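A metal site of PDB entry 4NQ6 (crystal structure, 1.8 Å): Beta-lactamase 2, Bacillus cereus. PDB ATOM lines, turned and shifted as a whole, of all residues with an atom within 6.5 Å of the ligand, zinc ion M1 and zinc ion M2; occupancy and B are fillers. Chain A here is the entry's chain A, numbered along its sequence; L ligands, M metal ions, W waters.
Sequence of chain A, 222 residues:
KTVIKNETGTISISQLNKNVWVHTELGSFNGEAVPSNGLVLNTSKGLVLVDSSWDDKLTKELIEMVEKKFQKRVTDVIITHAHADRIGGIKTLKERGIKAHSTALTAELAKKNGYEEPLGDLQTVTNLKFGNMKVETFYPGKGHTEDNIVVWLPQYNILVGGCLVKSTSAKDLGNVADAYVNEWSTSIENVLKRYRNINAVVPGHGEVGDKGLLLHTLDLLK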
ATOM      1  N   PHE A  29      27.343  18.001 -30.088  1.00  0.00           N
ATOM      2  CA  PHE A  29      27.745  18.476 -28.759  1.00  0.00           C
ATOM      3  C   PHE A  29      27.240  17.494 -27.659  1.00  0.00           C
ATOM      4  O   PHE A  29      27.342  16.284 -27.861  1.00  0.00           O
ATOM      5  CB  PHE A  29      27.302  19.952 -28.555  1.00  0.00           C
ATOM      6  CG  PHE A  29      28.137  20.702 -27.524  1.00  0.00           C
ATOM      7  CD1 PHE A  29      29.514  20.850 -27.701  1.00  0.00           C
ATOM      8  CD2 PHE A  29      27.538  21.282 -26.398  1.00  0.00           C
ATOM      9  CE1 PHE A  29      30.277  21.527 -26.760  1.00  0.00           C
ATOM     10  CE2 PHE A  29      28.299  21.952 -25.445  1.00  0.00           C
ATOM     11  CZ  PHE A  29      29.674  22.078 -25.626  1.00  0.00           C
ATOM     12  N   VAL A  34      23.634  20.013 -32.730  1.00  0.00           N
ATOM     13  CA  VAL A  34      23.636  21.446 -32.349  1.00  0.00           C
ATOM     14  C   VAL A  34      24.103  22.340 -33.492  1.00  0.00           C
ATOM     15  O   VAL A  34      25.224  22.162 -33.986  1.00  0.00           O
ATOM     16  CB  VAL A  34      24.583  21.727 -31.170  1.00  0.00           C
ATOM     17  CG1 VAL A  34      24.264  23.093 -30.554  1.00  0.00           C
ATOM     18  CG2 VAL A  34      24.533  20.597 -30.165  1.00  0.00           C
ATOM     19  N   PRO A  35      23.276  23.316 -33.901  1.00  0.00           N
ATOM     20  CA  PRO A  35      23.716  24.053 -35.070  1.00  0.00           C
ATOM     21  C   PRO A  35      24.631  25.221 -34.741  1.00  0.00           C
ATOM     22  O   PRO A  35      24.479  25.857 -33.686  1.00  0.00           O
ATOM     23  CB  PRO A  35      22.414  24.565 -35.674  1.00  0.00           C
ATOM     24  CG  PRO A  35      21.506  24.711 -34.512  1.00  0.00           C
ATOM     25  CD  PRO A  35      21.890  23.623 -33.555  1.00  0.00           C
ATOM     26  N   SER A  36      25.523  25.510 -35.687  1.00  0.00           N
ATOM     27  CA  SER A  36      26.504  26.577 -35.578  1.00  0.00           C
ATOM     28  C   SER A  36      26.429  27.415 -36.850  1.00  0.00           C
ATOM     29  O   SER A  36      26.461  26.848 -37.949  1.00  0.00           O
ATOM     30  CB  SER A  36      27.897  25.929 -35.421  1.00  0.00           C
ATOM     31  OG  SER A  36      28.926  26.900 -35.296  1.00  0.00           O
ATOM     32  N   TRP A  54      32.686  23.070 -37.037  1.00  0.00           N
ATOM     33  CA  TRP A  54      33.002  22.251 -35.849  1.00  0.00           C
ATOM     34  C   TRP A  54      34.308  21.470 -35.922  1.00  0.00           C
ATOM     35  O   TRP A  54      35.020  21.346 -34.938  1.00  0.00           O
ATOM     36  CB  TRP A  54      31.861  21.198 -35.589  1.00  0.00           C
ATOM     37  CG  TRP A  54      30.545  21.772 -35.210  1.00  0.00           C
ATOM     38  CD1 TRP A  54      29.538  22.134 -36.060  1.00  0.00           C
ATOM     39  CD2 TRP A  54      30.064  22.052 -33.872  1.00  0.00           C
ATOM     40  NE1 TRP A  54      28.468  22.636 -35.342  1.00  0.00           N
ATOM     41  CE2 TRP A  54      28.758  22.611 -34.003  1.00  0.00           C
ATOM     42  CE3 TRP A  54      30.605  21.898 -32.582  1.00  0.00           C
ATOM     43  CZ2 TRP A  54      27.988  23.015 -32.895  1.00  0.00           C
ATOM     44  CZ3 TRP A  54      29.822  22.284 -31.470  1.00  0.00           C
ATOM     45  CH2 TRP A  54      28.540  22.838 -31.650  1.00  0.00           C
ATOM     46  N   HIS A  81      36.369  33.168 -32.310  1.00  0.00           N
ATOM     47  CA  HIS A  81      37.056  32.860 -31.057  1.00  0.00           C
ATOM     48  C   HIS A  81      37.623  31.434 -31.101  1.00  0.00           C
ATOM     49  O   HIS A  81      37.521  30.742 -32.106  1.00  0.00           O
ATOM     50  CB  HIS A  81      36.170  33.089 -29.791  1.00  0.00           C
ATOM     51  CG  HIS A  81      34.956  32.220 -29.723  1.00  0.00           C
ATOM     52  ND1 HIS A  81      33.824  32.474 -30.442  1.00  0.00           N
ATOM     53  CD2 HIS A  81      34.668  31.131 -28.957  1.00  0.00           C
ATOM     54  CE1 HIS A  81      32.892  31.586 -30.149  1.00  0.00           C
ATOM     55  NE2 HIS A  81      33.383  30.762 -29.238  1.00  0.00           N
ATOM     56  N   ALA A  82      38.224  30.981 -29.994  1.00  0.00           N
ATOM     57  CA  ALA A  82      39.069  29.794 -29.997  1.00  0.00           C
ATOM     58  C   ALA A  82      38.386  28.543 -29.460  1.00  0.00           C
ATOM     59  O   ALA A  82      39.032  27.546 -29.210  1.00  0.00           O
ATOM     60  CB  ALA A  82      40.330  30.055 -29.208  1.00  0.00           C
ATOM     61  N   HIS A  83      37.100  28.544 -29.304  1.00  0.00           N
ATOM     62  CA  HIS A  83      36.410  27.304 -29.038  1.00  0.00           C
ATOM     63  C   HIS A  83      36.445  26.415 -30.277  1.00  0.00           C
ATOM     64  O   HIS A  83      36.368  26.908 -31.426  1.00  0.00           O
ATOM     65  CB  HIS A  83      34.959  27.529 -28.635  1.00  0.00           C
ATOM     66  CG  HIS A  83      34.790  27.873 -27.192  1.00  0.00           C
ATOM     67  ND1 HIS A  83      33.742  28.636 -26.719  1.00  0.00           N
ATOM     68  CD2 HIS A  83      35.627  27.663 -26.140  1.00  0.00           C
ATOM     69  CE1 HIS A  83      33.872  28.771 -25.417  1.00  0.00           C
ATOM     70  NE2 HIS A  83      35.005  28.199 -25.045  1.00  0.00           N
ATOM     71  N   ALA A  84      36.434  25.101 -30.008  1.00  0.00           N
ATOM     72  CA  ALA A  84      36.403  24.076 -31.022  1.00  0.00           C
ATOM     73  C   ALA A  84      35.354  24.348 -32.111  1.00  0.00           C
ATOM     74  O   ALA A  84      35.600  24.129 -33.322  1.00  0.00           O
ATOM     75  CB  ALA A  84      36.159  22.696 -30.370  1.00  0.00           C
ATOM     76  N   ASP A  85      34.188  24.844 -31.705  1.00  0.00           N
ATOM     77  CA  ASP A  85      33.128  25.171 -32.694  1.00  0.00           C
ATOM     78  C   ASP A  85      33.571  26.106 -33.858  1.00  0.00           C
ATOM     79  O   ASP A  85      33.113  25.989 -34.967  1.00  0.00           O
ATOM     80  CB  ASP A  85      31.945  25.838 -31.959  1.00  0.00           C
ATOM     81  CG  ASP A  85      30.807  26.164 -32.869  1.00  0.00           C
ATOM     82  OD1 ASP A  85      30.479  25.331 -33.678  1.00  0.00           O
ATOM     83  OD2 ASP A  85      30.205  27.253 -32.779  1.00  0.00           O
ATOM     84  N   ARG A  86      34.429  27.065 -33.524  1.00  0.00           N
ATOM     85  CA  ARG A  86      34.995  28.059 -34.490  1.00  0.00           C
ATOM     86  C   ARG A  86      36.382  27.677 -35.075  1.00  0.00           C
ATOM     87  O   ARG A  86      36.641  27.934 -36.233  1.00  0.00           O
ATOM     88  CB  ARG A  86      35.139  29.408 -33.751  1.00  0.00           C
ATOM     89  CG  ARG A  86      33.876  29.893 -33.049  1.00  0.00           C
ATOM     90  CD  ARG A  86      32.716  29.755 -34.006  1.00  0.00           C
ATOM     91  NE  ARG A  86      31.427  30.237 -33.603  1.00  0.00           N
ATOM     92  CZ  ARG A  86      30.334  30.111 -34.374  1.00  0.00           C
ATOM     93  NH1 ARG A  86      29.157  30.528 -33.960  1.00  0.00           N
ATOM     94  NH2 ARG A  86      30.400  29.589 -35.574  1.00  0.00           N
ATOM     95  N   HIS A 144      31.104  35.969 -23.955  1.00  0.00           N
ATOM     96  CA  HIS A 144      30.979  34.526 -24.094  1.00  0.00           C
ATOM     97  C   HIS A 144      32.350  33.811 -23.882  1.00  0.00           C
ATOM     98  O   HIS A 144      32.415  32.783 -23.265  1.00  0.00           O
ATOM     99  CB  HIS A 144      30.425  34.187 -25.464  1.00  0.00           C
ATOM    100  CG  HIS A 144      30.657  32.760 -25.855  1.00  0.00           C
ATOM    101  ND1 HIS A 144      29.939  31.721 -25.319  1.00  0.00           N
ATOM    102  CD2 HIS A 144      31.541  32.210 -26.717  1.00  0.00           C
ATOM    103  CE1 HIS A 144      30.323  30.597 -25.876  1.00  0.00           C
ATOM    104  NE2 HIS A 144      31.304  30.858 -26.708  1.00  0.00           N
ATOM    105  N   THR A 145      33.427  34.422 -24.390  1.00  0.00           N
ATOM    106  CA  THR A 145      34.792  34.065 -24.067  1.00  0.00           C
ATOM    107  C   THR A 145      35.595  35.348 -23.935  1.00  0.00           C
ATOM    108  O   THR A 145      35.115  36.441 -24.210  1.00  0.00           O
ATOM    109  CB  THR A 145      35.476  33.210 -25.165  1.00  0.00           C
ATOM    110  OG1 THR A 145      35.361  33.893 -26.413  1.00  0.00           O
ATOM    111  CG2 THR A 145      34.936  31.812 -25.224  1.00  0.00           C
ATOM    112  N   GLY A 162      28.417  36.157 -33.664  1.00  0.00           N
ATOM    113  CA  GLY A 162      29.107  35.013 -33.078  1.00  0.00           C
ATOM    114  C   GLY A 162      28.483  34.622 -31.733  1.00  0.00           C
ATOM    115  O   GLY A 162      27.308  34.984 -31.420  1.00  0.00           O
ATOM    116  N   CYS A 163      29.247  33.916 -30.908  1.00  0.00           N
ATOM    117  CA  CYS A 163      28.666  33.376 -29.690  1.00  0.00           C
ATOM    118  C   CYS A 163      28.416  34.413 -28.570  1.00  0.00           C
ATOM    119  O   CYS A 163      27.747  34.136 -27.614  1.00  0.00           O
ATOM    120  CB  CYS A 163      29.360  32.071 -29.261  1.00  0.00           C
ATOM    121  SG  CYS A 163      29.472  30.890 -30.643  1.00  0.00           S
ATOM    122  N   LEU A 164      28.934  35.635 -28.748  1.00  0.00           N
ATOM    123  CA  LEU A 164      28.611  36.768 -27.933  1.00  0.00           C
ATOM    124  C   LEU A 164      27.120  37.048 -27.946  1.00  0.00           C
ATOM    125  O   LEU A 164      26.601  37.658 -27.007  1.00  0.00           O
ATOM    126  CB  LEU A 164      29.378  38.000 -28.409  1.00  0.00           C
ATOM    127  CG  LEU A 164      29.329  39.258 -27.556  1.00  0.00           C
ATOM    128  CD1 LEU A 164      30.151  39.168 -26.266  1.00  0.00           C
ATOM    129  CD2 LEU A 164      29.724  40.448 -28.362  1.00  0.00           C
ATOM    130  N   LYS A 166      23.200  35.824 -28.435  1.00  0.00           N
ATOM    131  CA  LYS A 166      22.245  34.695 -28.344  1.00  0.00           C
ATOM    132  C   LYS A 166      21.027  34.869 -29.243  1.00  0.00           C
ATOM    133  O   LYS A 166      20.571  35.952 -29.452  1.00  0.00           O
ATOM    134  CB  LYS A 166      21.778  34.517 -26.876  1.00  0.00           C
ATOM    135  CG  LYS A 166      22.920  34.380 -25.866  1.00  0.00           C
ATOM    136  CD  LYS A 166      23.930  33.346 -26.276  1.00  0.00           C
ATOM    137  CE  LYS A 166      23.483  31.919 -26.046  1.00  0.00           C
ATOM    138  NZ  LYS A 166      24.689  31.025 -25.810  1.00  0.00           N
ATOM    139  N   LEU A 173      22.383  31.462 -21.027  1.00  0.00           N
ATOM    140  CA  LEU A 173      23.643  31.834 -21.654  1.00  0.00           C
ATOM    141  C   LEU A 173      24.475  30.696 -22.266  1.00  0.00           C
ATOM    142  O   LEU A 173      25.458  30.991 -22.951  1.00  0.00           O
ATOM    143  CB  LEU A 173      24.493  32.645 -20.709  1.00  0.00           C
ATOM    144  CG  LEU A 173      23.853  33.981 -20.288  1.00  0.00           C
ATOM    145  CD1 LEU A 173      24.559  34.475 -19.049  1.00  0.00           C
ATOM    146  CD2 LEU A 173      23.857  34.973 -21.427  1.00  0.00           C
ATOM    147  N   GLY A 174      24.063  29.425 -22.101  1.00  0.00           N
ATOM    148  CA  GLY A 174      24.828  28.318 -22.713  1.00  0.00           C
ATOM    149  C   GLY A 174      25.968  27.945 -21.781  1.00  0.00           C
ATOM    150  O   GLY A 174      25.856  28.106 -20.560  1.00  0.00           O
ATOM    151  N   ASN A 175      27.076  27.471 -22.309  1.00  0.00           N
ATOM    152  CA  ASN A 175      28.172  27.129 -21.407  1.00  0.00           C
ATOM    153  C   ASN A 175      28.934  28.397 -21.048  1.00  0.00           C
ATOM    154  O   ASN A 175      29.416  29.091 -21.927  1.00  0.00           O
ATOM    155  CB  ASN A 175      29.137  26.101 -21.997  1.00  0.00           C
ATOM    156  CG  ASN A 175      30.253  25.719 -21.033  1.00  0.00           C
ATOM    157  OD1 ASN A 175      30.095  24.823 -20.202  1.00  0.00           O
ATOM    158  ND2 ASN A 175      31.376  26.395 -21.142  1.00  0.00           N
ATOM    159  N   TRP A 184      30.379  40.845 -20.106  1.00  0.00           N
ATOM    160  CA  TRP A 184      29.592  40.539 -21.300  1.00  0.00           C
ATOM    161  C   TRP A 184      28.581  41.659 -21.600  1.00  0.00           C
ATOM    162  O   TRP A 184      28.352  42.044 -22.773  1.00  0.00           O
ATOM    163  CB  TRP A 184      28.905  39.192 -21.091  1.00  0.00           C
ATOM    164  CG  TRP A 184      28.419  38.461 -22.282  1.00  0.00           C
ATOM    165  CD1 TRP A 184      28.039  38.992 -23.499  1.00  0.00           C
ATOM    166  CD2 TRP A 184      28.142  37.052 -22.366  1.00  0.00           C
ATOM    167  NE1 TRP A 184      27.571  38.003 -24.309  1.00  0.00           N
ATOM    168  CE2 TRP A 184      27.632  36.799 -23.651  1.00  0.00           C
ATOM    169  CE3 TRP A 184      28.259  35.977 -21.467  1.00  0.00           C
ATOM    170  CZ2 TRP A 184      27.208  35.532 -24.064  1.00  0.00           C
ATOM    171  CZ3 TRP A 184      27.878  34.723 -21.891  1.00  0.00           C
ATOM    172  CH2 TRP A 184      27.372  34.499 -23.183  1.00  0.00           C
ATOM    173  N   GLY A 204      25.674  33.282 -32.989  1.00  0.00           N
ATOM    174  CA  GLY A 204      26.598  32.145 -33.133  1.00  0.00           C
ATOM    175  C   GLY A 204      25.821  30.849 -33.486  1.00  0.00           C
ATOM    176  O   GLY A 204      26.296  30.011 -34.230  1.00  0.00           O
ATOM    177  N   HIS A 205      24.669  30.703 -32.845  1.00  0.00           N
ATOM    178  CA  HIS A 205      23.767  29.596 -32.993  1.00  0.00           C
ATOM    179  C   HIS A 205      22.328  30.160 -33.091  1.00  0.00           C
ATOM    180  O   HIS A 205      21.922  31.022 -32.288  1.00  0.00           O
ATOM    181  CB  HIS A 205      23.877  28.693 -31.755  1.00  0.00           C
ATOM    182  CG  HIS A 205      25.296  28.290 -31.418  1.00  0.00           C
ATOM    183  ND1 HIS A 205      25.968  27.295 -32.093  1.00  0.00           N
ATOM    184  CD2 HIS A 205      26.182  28.794 -30.521  1.00  0.00           C
ATOM    185  CE1 HIS A 205      27.187  27.169 -31.616  1.00  0.00           C
ATOM    186  NE2 HIS A 205      27.347  28.060 -30.655  1.00  0.00           N
HETATM  187  O1  LIG L   1      26.821  29.027 -25.942  1.00  0.00           O
HETATM  188  N1  LIG L   1      28.788  26.726 -27.946  1.00  0.00           N
HETATM  189  C1  LIG L   1      27.449  28.620 -26.923  1.00  0.00           C
HETATM  190  O2  LIG L   1      27.890  29.359 -27.856  1.00  0.00           O
HETATM  191  C2  LIG L   1      27.723  27.057 -26.930  1.00  0.00           C
HETATM  192  C3  LIG L   1      26.442  26.197 -27.136  1.00  0.00           C
HETATM  193  S1  LIG L   1      26.727  25.274 -28.641  1.00  0.00           S
HETATM  194  C4  LIG L   1      28.478  25.559 -28.850  1.00  0.00           C
HETATM  195  C5  LIG L   1      29.187  24.310 -28.393  1.00  0.00           C
HETATM  196  S2  LIG L   1      29.567  24.837 -26.716  1.00  0.00           S
HETATM  197  C6  LIG L   1      30.029  26.477 -27.182  1.00  0.00           C
HETATM  198  C7  LIG L   1      31.241  26.540 -28.057  1.00  0.00           C
HETATM  199  S3  LIG L   1      31.014  27.989 -29.153  1.00  0.00           S
HETATM  200 ZN    ZN M   1      32.304  29.511 -27.951  1.00  0.00          ZN
HETATM  201 ZN    ZN M   2      28.903  28.906 -29.526  1.00  0.00          ZN
HETATM  202  O   HOH W   1      33.115  24.216 -29.094  1.00  0.00           O
HETATM  203  O   HOH W   2      26.360  31.690 -28.027  1.00  0.00           O
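O1 of the ligand lies within salt-bridge range of NZ of Lys 166.
The side-chain carboxylate of Asp 85 lies close to a sulfur (S3) of the ligand, 3.8 Å away.
The backbone carbonyl oxygen of Leu 173 is in hydrogen-bond range of the side-chain amino group of Lys 166, 3.0 Å away.
SG of Cys 163 sits close to NH1 of Arg 86, 3.4 Å away.
OD1 of Asp 85 is in hydrogen-bond range of OG of Ser 36, at 2.7 Å.
The backbone carbonyl oxygen (O) of Pro 35 lies within hydrogen-bond range of a ring nitrogen (ND1) of His 205.
The side-chain carboxylate of Asp 85 lies within salt-bridge range of the guanidinium group of Arg 86.
Residues that only touch the ligand: Phe 29 (3.0 Å), Trp 54 (3.6 Å), Val 34 (3.8 Å), Leu 173 (3.8 Å), Gly 174 (3.9 Å) and Asn 175 (3.96 Å).
Three residues have an atom within 4 Å of zinc ion M1: His 81, His 83 and His 144.
Merely in contact with zinc ion M2: Asp 85 (3.9 Å).
Of the 23 residues printed, 3 come within 4 Å of zinc ion M2.
Zinc ion M1 is bound by ND1 of His 83, NE2 of His 144, NE2 of His 81 and S3 of the ligand.
Zinc ion M2 is bound by O2 of the ligand (2.0 Å), NE2 of His 205 (2.1 Å), S3 of the ligand (2.3 Å) and SG of Cys 163 (2.3 Å).
Zinc ion M2 has four donor atoms within binding distance.
Slightly farther from zinc ion M2 lies a nitrogen (N1) of the ligand (2.7 Å).
Water W2 lies within hydrogen-bond range of the backbone carbonyl oxygen (O) of Cys 163 (2.8 Å), the side-chain amino group (NZ) of Lys 166 (2.9 Å) and an oxygen (O1) of the ligand (3.4 Å).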
